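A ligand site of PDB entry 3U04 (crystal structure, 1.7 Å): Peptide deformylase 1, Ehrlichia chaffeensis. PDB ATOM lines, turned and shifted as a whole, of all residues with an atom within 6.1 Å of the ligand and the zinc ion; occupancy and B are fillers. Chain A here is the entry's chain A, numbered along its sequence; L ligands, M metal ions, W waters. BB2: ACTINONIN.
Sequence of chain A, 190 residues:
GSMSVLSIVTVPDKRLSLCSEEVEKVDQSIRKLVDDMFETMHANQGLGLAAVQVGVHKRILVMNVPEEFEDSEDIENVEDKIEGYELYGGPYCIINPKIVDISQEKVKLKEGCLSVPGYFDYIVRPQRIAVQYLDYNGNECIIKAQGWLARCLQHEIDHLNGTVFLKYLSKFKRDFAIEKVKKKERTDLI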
ATOM      1  N   ASN A  44     -39.815  -8.605  -0.610  1.00  0.00           N
ATOM      2  CA  ASN A  44     -38.865  -8.285   0.450  1.00  0.00           C
ATOM      3  C   ASN A  44     -38.176  -6.934   0.280  1.00  0.00           C
ATOM      4  O   ASN A  44     -37.274  -6.604   1.047  1.00  0.00           O
ATOM      5  CB  ASN A  44     -37.819  -9.411   0.553  1.00  0.00           C
ATOM      6  CG  ASN A  44     -38.328 -10.571   1.347  1.00  0.00           C
ATOM      7  OD1 ASN A  44     -38.463 -10.481   2.579  1.00  0.00           O
ATOM      8  ND2 ASN A  44     -38.677 -11.678   0.667  1.00  0.00           N
ATOM      9  N   GLN A  45     -38.628  -6.154  -0.700  1.00  0.00           N
ATOM     10  CA  GLN A  45     -38.072  -4.832  -0.970  1.00  0.00           C
ATOM     11  C   GLN A  45     -36.586  -4.864  -1.283  1.00  0.00           C
ATOM     12  O   GLN A  45     -35.862  -3.970  -0.851  1.00  0.00           O
ATOM     13  CB  GLN A  45     -38.339  -3.881   0.235  1.00  0.00           C
ATOM     14  CG  GLN A  45     -39.811  -3.736   0.534  1.00  0.00           C
ATOM     15  CD  GLN A  45     -40.530  -2.969  -0.565  1.00  0.00           C
ATOM     16  OE1 GLN A  45     -40.056  -1.920  -1.011  1.00  0.00           O
ATOM     17  NE2 GLN A  45     -41.655  -3.512  -1.029  1.00  0.00           N
ATOM     18  N   GLY A  46     -36.155  -5.915  -1.975  1.00  0.00           N
ATOM     19  CA  GLY A  46     -34.730  -6.080  -2.340  1.00  0.00           C
ATOM     20  C   GLY A  46     -34.352  -5.512  -3.694  1.00  0.00           C
ATOM     21  O   GLY A  46     -35.183  -5.368  -4.604  1.00  0.00           O
ATOM     22  N   LEU A  47     -33.054  -5.252  -3.865  1.00  0.00           N
ATOM     23  CA  LEU A  47     -32.476  -4.868  -5.143  1.00  0.00           C
ATOM     24  C   LEU A  47     -32.019  -6.088  -5.985  1.00  0.00           C
ATOM     25  O   LEU A  47     -31.760  -5.982  -7.177  1.00  0.00           O
ATOM     26  CB  LEU A  47     -31.257  -3.996  -4.864  1.00  0.00           C
ATOM     27  CG  LEU A  47     -31.441  -2.594  -4.308  1.00  0.00           C
ATOM     28  CD1 LEU A  47     -30.057  -2.042  -3.890  1.00  0.00           C
ATOM     29  CD2 LEU A  47     -32.102  -1.743  -5.371  1.00  0.00           C
ATOM     30  N   GLY A  48     -31.855  -7.228  -5.324  1.00  0.00           N
ATOM     31  CA  GLY A  48     -31.424  -8.444  -5.978  1.00  0.00           C
ATOM     32  C   GLY A  48     -31.710  -9.626  -5.084  1.00  0.00           C
ATOM     33  O   GLY A  48     -32.153  -9.440  -3.949  1.00  0.00           O
ATOM     34  N   LEU A  49     -31.415 -10.829  -5.590  1.00  0.00           N
ATOM     35  CA  LEU A  49     -31.593 -12.046  -4.816  1.00  0.00           C
ATOM     36  C   LEU A  49     -30.844 -13.172  -5.491  1.00  0.00           C
ATOM     37  O   LEU A  49     -30.787 -13.238  -6.717  1.00  0.00           O
ATOM     38  CB  LEU A  49     -33.101 -12.410  -4.720  1.00  0.00           C
ATOM     39  CG  LEU A  49     -33.536 -13.469  -3.709  1.00  0.00           C
ATOM     40  CD1 LEU A  49     -33.409 -12.932  -2.287  1.00  0.00           C
ATOM     41  CD2 LEU A  49     -34.983 -13.890  -3.984  1.00  0.00           C
ATOM     42  N   ALA A  50     -30.224 -14.026  -4.686  1.00  0.00           N
ATOM     43  CA  ALA A  50     -29.524 -15.191  -5.191  1.00  0.00           C
ATOM     44  C   ALA A  50     -30.297 -16.445  -4.868  1.00  0.00           C
ATOM     45  O   ALA A  50     -30.967 -16.507  -3.847  1.00  0.00           O
ATOM     46  CB  ALA A  50     -28.111 -15.263  -4.591  1.00  0.00           C
ATOM     47  N   GLN A  53     -30.345 -18.116  -1.379  1.00  0.00           N
ATOM     48  CA  GLN A  53     -31.141 -17.427  -0.385  1.00  0.00           C
ATOM     49  C   GLN A  53     -32.569 -17.953  -0.339  1.00  0.00           C
ATOM     50  O   GLN A  53     -33.264 -17.658   0.641  1.00  0.00           O
ATOM     51  CB  GLN A  53     -31.157 -15.926  -0.669  1.00  0.00           C
ATOM     52  CG  GLN A  53     -29.805 -15.272  -0.531  1.00  0.00           C
ATOM     53  CD  GLN A  53     -29.903 -13.793  -0.742  1.00  0.00           C
ATOM     54  OE1 GLN A  53     -29.899 -13.339  -1.878  1.00  0.00           O
ATOM     55  NE2 GLN A  53     -30.100 -13.031   0.348  1.00  0.00           N
ATOM     56  N   LEU A 109     -19.617   1.540   0.332  1.00  0.00           N
ATOM     57  CA  LEU A 109     -21.064   1.787   0.350  1.00  0.00           C
ATOM     58  C   LEU A 109     -21.719   0.947   1.454  1.00  0.00           C
ATOM     59  O   LEU A 109     -21.189  -0.081   1.866  1.00  0.00           O
ATOM     60  CB  LEU A 109     -21.681   1.410  -0.980  1.00  0.00           C
ATOM     61  CG  LEU A 109     -21.335   2.284  -2.193  1.00  0.00           C
ATOM     62  CD1 LEU A 109     -21.854   1.607  -3.492  1.00  0.00           C
ATOM     63  CD2 LEU A 109     -21.863   3.702  -2.032  1.00  0.00           C
ATOM     64  N   LYS A 110     -22.860   1.402   1.928  1.00  0.00           N
ATOM     65  CA  LYS A 110     -23.600   0.719   2.968  1.00  0.00           C
ATOM     66  C   LYS A 110     -24.407  -0.413   2.328  1.00  0.00           C
ATOM     67  O   LYS A 110     -25.060  -0.204   1.286  1.00  0.00           O
ATOM     68  CB  LYS A 110     -24.549   1.685   3.648  1.00  0.00           C
ATOM     69  CG  LYS A 110     -25.225   1.050   4.849  1.00  0.00           C
ATOM     70  CD  LYS A 110     -26.004   2.041   5.690  1.00  0.00           C
ATOM     71  CE  LYS A 110     -27.417   2.217   5.216  1.00  0.00           C
ATOM     72  NZ  LYS A 110     -28.184   3.051   6.198  1.00  0.00           N
ATOM     73  N   GLU A 111     -24.344  -1.579   2.950  1.00  0.00           N
ATOM     74  CA  GLU A 111     -25.115  -2.748   2.486  1.00  0.00           C
ATOM     75  C   GLU A 111     -25.908  -3.367   3.593  1.00  0.00           C
ATOM     76  O   GLU A 111     -25.476  -3.400   4.730  1.00  0.00           O
ATOM     77  CB  GLU A 111     -24.167  -3.847   1.981  1.00  0.00           C
ATOM     78  CG  GLU A 111     -23.351  -3.466   0.817  1.00  0.00           C
ATOM     79  CD  GLU A 111     -22.542  -4.601   0.215  1.00  0.00           C
ATOM     80  OE1 GLU A 111     -22.934  -5.820   0.331  1.00  0.00           O
ATOM     81  OE2 GLU A 111     -21.524  -4.236  -0.380  1.00  0.00           O
ATOM     82  N   GLY A 112     -27.064  -3.934   3.222  1.00  0.00           N
ATOM     83  CA  GLY A 112     -27.713  -4.926   4.035  1.00  0.00           C
ATOM     84  C   GLY A 112     -27.978  -6.125   3.170  1.00  0.00           C
ATOM     85  O   GLY A 112     -27.614  -6.157   1.982  1.00  0.00           O
ATOM     86  N   CYS A 113     -28.579  -7.131   3.787  1.00  0.00           N
ATOM     87  CA  CYS A 113     -28.830  -8.416   3.102  1.00  0.00           C
ATOM     88  C   CYS A 113     -30.088  -9.027   3.635  1.00  0.00           C
ATOM     89  O   CYS A 113     -30.295  -9.053   4.874  1.00  0.00           O
ATOM     90  CB  CYS A 113     -27.689  -9.383   3.394  1.00  0.00           C
ATOM     91  SG  CYS A 113     -27.716 -11.002   2.599  1.00  0.00           S
ATOM     92  N   LEU A 114     -30.878  -9.633   2.756  1.00  0.00           N
ATOM     93  CA  LEU A 114     -32.090 -10.314   3.224  1.00  0.00           C
ATOM     94  C   LEU A 114     -31.823 -11.519   4.139  1.00  0.00           C
ATOM     95  O   LEU A 114     -32.675 -11.888   4.967  1.00  0.00           O
ATOM     96  CB  LEU A 114     -32.977 -10.735   2.023  1.00  0.00           C
ATOM     97  CG  LEU A 114     -33.446  -9.531   1.181  1.00  0.00           C
ATOM     98  CD1 LEU A 114     -34.214 -10.020  -0.026  1.00  0.00           C
ATOM     99  CD2 LEU A 114     -34.326  -8.607   1.995  1.00  0.00           C
ATOM    100  N   SER A 115     -30.639 -12.104   4.025  1.00  0.00           N
ATOM    101  CA  SER A 115     -30.212 -13.223   4.855  1.00  0.00           C
ATOM    102  C   SER A 115     -29.574 -12.782   6.176  1.00  0.00           C
ATOM    103  O   SER A 115     -29.249 -13.610   7.020  1.00  0.00           O
ATOM    104  CB  SER A 115     -29.223 -14.098   4.084  1.00  0.00           C
ATOM    105  OG  SER A 115     -29.833 -14.585   2.931  1.00  0.00           O
ATOM    106  N   TYR A 119     -29.498  -5.814   9.768  1.00  0.00           N
ATOM    107  CA  TYR A 119     -28.108  -5.425  10.034  1.00  0.00           C
ATOM    108  C   TYR A 119     -27.547  -4.756   8.798  1.00  0.00           C
ATOM    109  O   TYR A 119     -27.581  -5.335   7.708  1.00  0.00           O
ATOM    110  CB  TYR A 119     -27.221  -6.643  10.423  1.00  0.00           C
ATOM    111  CG  TYR A 119     -25.859  -6.229  10.851  1.00  0.00           C
ATOM    112  CD1 TYR A 119     -25.626  -5.806  12.135  1.00  0.00           C
ATOM    113  CD2 TYR A 119     -24.788  -6.233   9.955  1.00  0.00           C
ATOM    114  CE1 TYR A 119     -24.372  -5.365  12.528  1.00  0.00           C
ATOM    115  CE2 TYR A 119     -23.533  -5.792  10.349  1.00  0.00           C
ATOM    116  CZ  TYR A 119     -23.329  -5.369  11.634  1.00  0.00           C
ATOM    117  OH  TYR A 119     -22.095  -4.904  12.032  1.00  0.00           O
ATOM    118  N   PHE A 120     -27.008  -3.561   8.974  1.00  0.00           N
ATOM    119  CA  PHE A 120     -26.340  -2.838   7.873  1.00  0.00           C
ATOM    120  C   PHE A 120     -24.898  -2.504   8.227  1.00  0.00           C
ATOM    121  O   PHE A 120     -24.588  -2.212   9.367  1.00  0.00           O
ATOM    122  CB  PHE A 120     -27.075  -1.545   7.559  1.00  0.00           C
ATOM    123  CG  PHE A 120     -28.446  -1.733   7.024  1.00  0.00           C
ATOM    124  CD1 PHE A 120     -29.507  -1.985   7.900  1.00  0.00           C
ATOM    125  CD2 PHE A 120     -28.691  -1.683   5.643  1.00  0.00           C
ATOM    126  CE1 PHE A 120     -30.799  -2.187   7.396  1.00  0.00           C
ATOM    127  CE2 PHE A 120     -29.968  -1.879   5.157  1.00  0.00           C
ATOM    128  CZ  PHE A 120     -31.015  -2.131   6.033  1.00  0.00           C
ATOM    129  N   ARG A 125     -15.862  -2.357  -2.178  1.00  0.00           N
ATOM    130  CA  ARG A 125     -15.862  -3.201  -3.369  1.00  0.00           C
ATOM    131  C   ARG A 125     -15.447  -2.390  -4.598  1.00  0.00           C
ATOM    132  O   ARG A 125     -15.646  -1.188  -4.619  1.00  0.00           O
ATOM    133  CB  ARG A 125     -17.249  -3.772  -3.677  1.00  0.00           C
ATOM    134  CG  ARG A 125     -17.908  -4.562  -2.525  1.00  0.00           C
ATOM    135  CD  ARG A 125     -19.143  -5.196  -3.072  1.00  0.00           C
ATOM    136  NE  ARG A 125     -19.998  -5.842  -2.058  1.00  0.00           N
ATOM    137  CZ  ARG A 125     -19.949  -7.138  -1.731  1.00  0.00           C
ATOM    138  NH1 ARG A 125     -19.159  -8.005  -2.349  1.00  0.00           N
ATOM    139  NH2 ARG A 125     -20.790  -7.570  -0.791  1.00  0.00           N
ATOM    140  N   TRP A 148     -24.782   1.620  -8.019  1.00  0.00           N
ATOM    141  CA  TRP A 148     -25.503   0.629  -7.254  1.00  0.00           C
ATOM    142  C   TRP A 148     -25.765  -0.653  -8.002  1.00  0.00           C
ATOM    143  O   TRP A 148     -25.934  -1.695  -7.385  1.00  0.00           O
ATOM    144  CB  TRP A 148     -26.810   1.190  -6.720  1.00  0.00           C
ATOM    145  CG  TRP A 148     -26.606   2.158  -5.585  1.00  0.00           C
ATOM    146  CD1 TRP A 148     -26.668   3.559  -5.608  1.00  0.00           C
ATOM    147  CD2 TRP A 148     -26.231   1.829  -4.223  1.00  0.00           C
ATOM    148  NE1 TRP A 148     -26.394   4.086  -4.368  1.00  0.00           N
ATOM    149  CE2 TRP A 148     -26.140   3.091  -3.492  1.00  0.00           C
ATOM    150  CE3 TRP A 148     -26.016   0.658  -3.544  1.00  0.00           C
ATOM    151  CZ2 TRP A 148     -25.824   3.137  -2.133  1.00  0.00           C
ATOM    152  CZ3 TRP A 148     -25.707   0.712  -2.187  1.00  0.00           C
ATOM    153  CH2 TRP A 148     -25.612   1.922  -1.504  1.00  0.00           C
ATOM    154  N   ARG A 151     -22.665  -2.649  -7.481  1.00  0.00           N
ATOM    155  CA  ARG A 151     -22.649  -3.045  -6.071  1.00  0.00           C
ATOM    156  C   ARG A 151     -23.557  -4.242  -5.779  1.00  0.00           C
ATOM    157  O   ARG A 151     -23.146  -5.218  -5.189  1.00  0.00           O
ATOM    158  CB  ARG A 151     -23.048  -1.841  -5.185  1.00  0.00           C
ATOM    159  CG  ARG A 151     -23.183  -2.166  -3.685  1.00  0.00           C
ATOM    160  CD  ARG A 151     -22.004  -2.876  -3.095  1.00  0.00           C
ATOM    161  NE  ARG A 151     -20.778  -2.053  -3.282  1.00  0.00           N
ATOM    162  CZ  ARG A 151     -19.986  -1.598  -2.316  1.00  0.00           C
ATOM    163  NH1 ARG A 151     -20.208  -1.891  -1.030  1.00  0.00           N
ATOM    164  NH2 ARG A 151     -18.945  -0.819  -2.679  1.00  0.00           N
ATOM    165  N   CYS A 152     -24.781  -4.182  -6.270  1.00  0.00           N
ATOM    166  CA  CYS A 152     -25.715  -5.281  -6.121  1.00  0.00           C
ATOM    167  C   CYS A 152     -25.193  -6.560  -6.761  1.00  0.00           C
ATOM    168  O   CYS A 152     -25.293  -7.625  -6.171  1.00  0.00           O
ATOM    169  CB  CYS A 152     -27.066  -4.898  -6.669  1.00  0.00           C
ATOM    170  SG  CYS A 152     -28.328  -6.201  -6.506  1.00  0.00           S
ATOM    171  N   HIS A 155     -22.559  -8.248  -4.691  1.00  0.00           N
ATOM    172  CA  HIS A 155     -23.163  -8.821  -3.481  1.00  0.00           C
ATOM    173  C   HIS A 155     -23.839 -10.117  -3.849  1.00  0.00           C
ATOM    174  O   HIS A 155     -23.637 -11.141  -3.172  1.00  0.00           O
ATOM    175  CB  HIS A 155     -24.100  -7.791  -2.883  1.00  0.00           C
ATOM    176  CG  HIS A 155     -24.910  -8.266  -1.712  1.00  0.00           C
ATOM    177  ND1 HIS A 155     -24.813  -7.681  -0.501  1.00  0.00           N
ATOM    178  CD2 HIS A 155     -25.901  -9.229  -1.600  1.00  0.00           C
ATOM    179  CE1 HIS A 155     -25.674  -8.285   0.355  1.00  0.00           C
ATOM    180  NE2 HIS A 155     -26.345  -9.225  -0.307  1.00  0.00           N
ATOM    181  N   GLU A 156     -24.534 -10.163  -4.981  1.00  0.00           N
ATOM    182  CA  GLU A 156     -25.269 -11.385  -5.400  1.00  0.00           C
ATOM    183  C   GLU A 156     -24.254 -12.485  -5.835  1.00  0.00           C
ATOM    184  O   GLU A 156     -24.393 -13.672  -5.458  1.00  0.00           O
ATOM    185  CB  GLU A 156     -26.258 -11.110  -6.539  1.00  0.00           C
ATOM    186  CG  GLU A 156     -27.379 -10.092  -6.232  1.00  0.00           C
ATOM    187  CD  GLU A 156     -28.152 -10.343  -4.952  1.00  0.00           C
ATOM    188  OE1 GLU A 156     -28.180 -11.490  -4.467  1.00  0.00           O
ATOM    189  OE2 GLU A 156     -28.704  -9.341  -4.427  1.00  0.00           O
ATOM    190  N   HIS A 159     -22.910 -14.390  -2.970  1.00  0.00           N
ATOM    191  CA  HIS A 159     -23.783 -15.415  -2.418  1.00  0.00           C
ATOM    192  C   HIS A 159     -23.619 -16.737  -3.153  1.00  0.00           C
ATOM    193  O   HIS A 159     -23.732 -17.810  -2.540  1.00  0.00           O
ATOM    194  CB  HIS A 159     -25.248 -15.014  -2.528  1.00  0.00           C
ATOM    195  CG  HIS A 159     -25.756 -14.126  -1.460  1.00  0.00           C
ATOM    196  ND1 HIS A 159     -25.764 -14.480  -0.135  1.00  0.00           N
ATOM    197  CD2 HIS A 159     -26.417 -12.917  -1.533  1.00  0.00           C
ATOM    198  CE1 HIS A 159     -26.365 -13.512   0.580  1.00  0.00           C
ATOM    199  NE2 HIS A 159     -26.752 -12.546  -0.270  1.00  0.00           N
ATOM    200  N   PHE A 165     -22.036 -10.876   3.258  1.00  0.00           N
ATOM    201  CA  PHE A 165     -21.260  -9.634   3.345  1.00  0.00           C
ATOM    202  C   PHE A 165     -20.588  -9.455   4.700  1.00  0.00           C
ATOM    203  O   PHE A 165     -19.654  -8.697   4.818  1.00  0.00           O
ATOM    204  CB  PHE A 165     -22.069  -8.379   2.952  1.00  0.00           C
ATOM    205  CG  PHE A 165     -22.998  -7.849   4.031  1.00  0.00           C
ATOM    206  CD1 PHE A 165     -24.138  -8.545   4.374  1.00  0.00           C
ATOM    207  CD2 PHE A 165     -22.765  -6.627   4.651  1.00  0.00           C
ATOM    208  CE1 PHE A 165     -25.037  -8.050   5.358  1.00  0.00           C
ATOM    209  CE2 PHE A 165     -23.627  -6.150   5.648  1.00  0.00           C
ATOM    210  CZ  PHE A 165     -24.754  -6.863   5.986  1.00  0.00           C
HETATM  211  C5  BB2 L   1     -30.666  -8.123  -1.132  1.00  0.00           C
HETATM  212  C3  BB2 L   1     -29.911  -9.374  -0.852  1.00  0.00           C
HETATM  213  O4  BB2 L   1     -29.590  -9.832   0.269  1.00  0.00           O
HETATM  214  N1  BB2 L   1     -29.450  -9.967  -1.942  1.00  0.00           N
HETATM  215  O2  BB2 L   1     -28.570 -10.984  -1.769  1.00  0.00           O
HETATM  216  C6  BB2 L   1     -29.748  -6.885  -1.061  1.00  0.00           C
HETATM  217  C12 BB2 L   1     -30.597  -5.715  -0.738  1.00  0.00           C
HETATM  218  O13 BB2 L   1     -31.553  -5.432  -1.453  1.00  0.00           O
HETATM  219  C7  BB2 L   1     -29.068  -6.610  -2.385  1.00  0.00           C
HETATM  220  C8  BB2 L   1     -28.268  -5.288  -2.426  1.00  0.00           C
HETATM  221  C9  BB2 L   1     -26.826  -5.551  -2.074  1.00  0.00           C
HETATM  222  C10 BB2 L   1     -25.844  -4.367  -2.136  1.00  0.00           C
HETATM  223  C11 BB2 L   1     -26.425  -2.996  -1.885  1.00  0.00           C
HETATM  224  N14 BB2 L   1     -30.237  -5.009   0.331  1.00  0.00           N
HETATM  225  C15 BB2 L   1     -30.850  -3.712   0.658  1.00  0.00           C
HETATM  226  C16 BB2 L   1     -31.759  -3.795   1.884  1.00  0.00           C
HETATM  227  C18 BB2 L   1     -33.065  -4.525   1.536  1.00  0.00           C
HETATM  228  C17 BB2 L   1     -31.142  -4.531   3.062  1.00  0.00           C
HETATM  229  C19 BB2 L   1     -29.744  -2.668   0.745  1.00  0.00           C
HETATM  230  O20 BB2 L   1     -28.653  -3.017   1.160  1.00  0.00           O
HETATM  231  N21 BB2 L   1     -29.962  -1.418   0.284  1.00  0.00           N
HETATM  232  C22 BB2 L   1     -28.922  -0.373   0.302  1.00  0.00           C
HETATM  233  C23 BB2 L   1     -31.208  -0.919  -0.345  1.00  0.00           C
HETATM  234  C24 BB2 L   1     -30.989   0.573  -0.586  1.00  0.00           C
HETATM  235  C25 BB2 L   1     -29.477   0.766  -0.560  1.00  0.00           C
HETATM  236  C26 BB2 L   1     -28.633   0.095   1.715  1.00  0.00           C
HETATM  237  O27 BB2 L   1     -27.589   1.100   1.672  1.00  0.00           O
HETATM  238 ZN    ZN M   1     -27.667 -10.703   0.286  1.00  0.00          ZN
HETATM  239  O   HOH W   1     -26.704   3.880   1.395  1.00  0.00           O
HETATM  240  O   HOH W   2     -24.602 -10.858   1.926  1.00  0.00           O
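A ring nitrogen (NE2) of His 155 binds the zinc ion, 2.1 Å away. The zinc ion is bound by O4 of the ligand, 2.1 Å away. The zinc ion is bound by NE2 of His 159 (2.1 Å). The zinc ion is bound by O2 of the ligand (2.3 Å). SG of Cys 113 binds the zinc ion (2.3 Å). The zinc ion has five donor atoms within binding distance.
Residues that only touch the zinc ion: Gln 53. Along chain A the residues within 4 Å of the zinc ion span positions 53 to 159.
The side-chain sulfur of Cys 152 sits at hydrogen-bond distance from the side-chain carboxylate of Glu 156 (3.8 Å). N of Leu 49 is in hydrogen-bond range of OE2 of Glu 156, 3.3 Å away. OE1 of Glu 156 lies within hydrogen-bond range of N of Ala 50 (3.3 Å). OG of Ser 115 sits at hydrogen-bond distance from NE2 of Gln 53, at 3.0 Å. OE1 of Gln 53 sits at hydrogen-bond distance from N of Ala 50 (2.9 Å). The backbone carbonyl oxygen (O) of Leu 47 sits at hydrogen-bond distance from the side-chain sulfur (SG) of Cys 152 (3.5 Å). The side-chain carboxylate (OE2) of Glu 111 is in salt-bridge range of the guanidinium group (NH1) of Arg 151. The guanidinium group of Arg 125 lies within salt-bridge range of the side-chain carboxylate of Glu 111 (2.8 Å).
Merely in contact with the ligand: Gly 46 (3.4 Å), Phe 120 (3.6 Å), Glu 111 (3.7 Å), Gln 45 (3.7 Å), Arg 151 (3.8 Å) and Trp 148 (3.8 Å). Hydrophobic or aromatic side chains that line the ligand: Leu 47, Leu 114, Phe 120, Trp 148, His 155 and His 159. The nearest printed residue that does not touch the ligand is Cys 152 (4.1 Å).
A nitrogen (N1) of the ligand sits at hydrogen-bond distance from the side-chain carboxylate of Glu 156 (2.7 Å). The side-chain amide oxygen of Gln 53 is in hydrogen-bond range of a nitrogen (N1) of the ligand. An oxygen (O20) of the ligand lies within hydrogen-bond range of the backbone NH (N) of Gly 112 (2.8 Å). A nitrogen (N14) of the ligand is in hydrogen-bond range of the backbone carbonyl oxygen (O) of Gly 112 (3.3 Å). The backbone NH (N) of Leu 114 sits close to an oxygen (O4) of the ligand, at 2.8 Å. The backbone NH (N) of Leu 47 is in hydrogen-bond range of an oxygen (O13) of the ligand, 2.8 Å away. An oxygen (O27) of the ligand sits at hydrogen-bond distance from the backbone carbonyl oxygen of Lys 110. The backbone carbonyl oxygen of Gly 48 sits at hydrogen-bond distance from a nitrogen (N1) of the ligand (3.4 Å).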
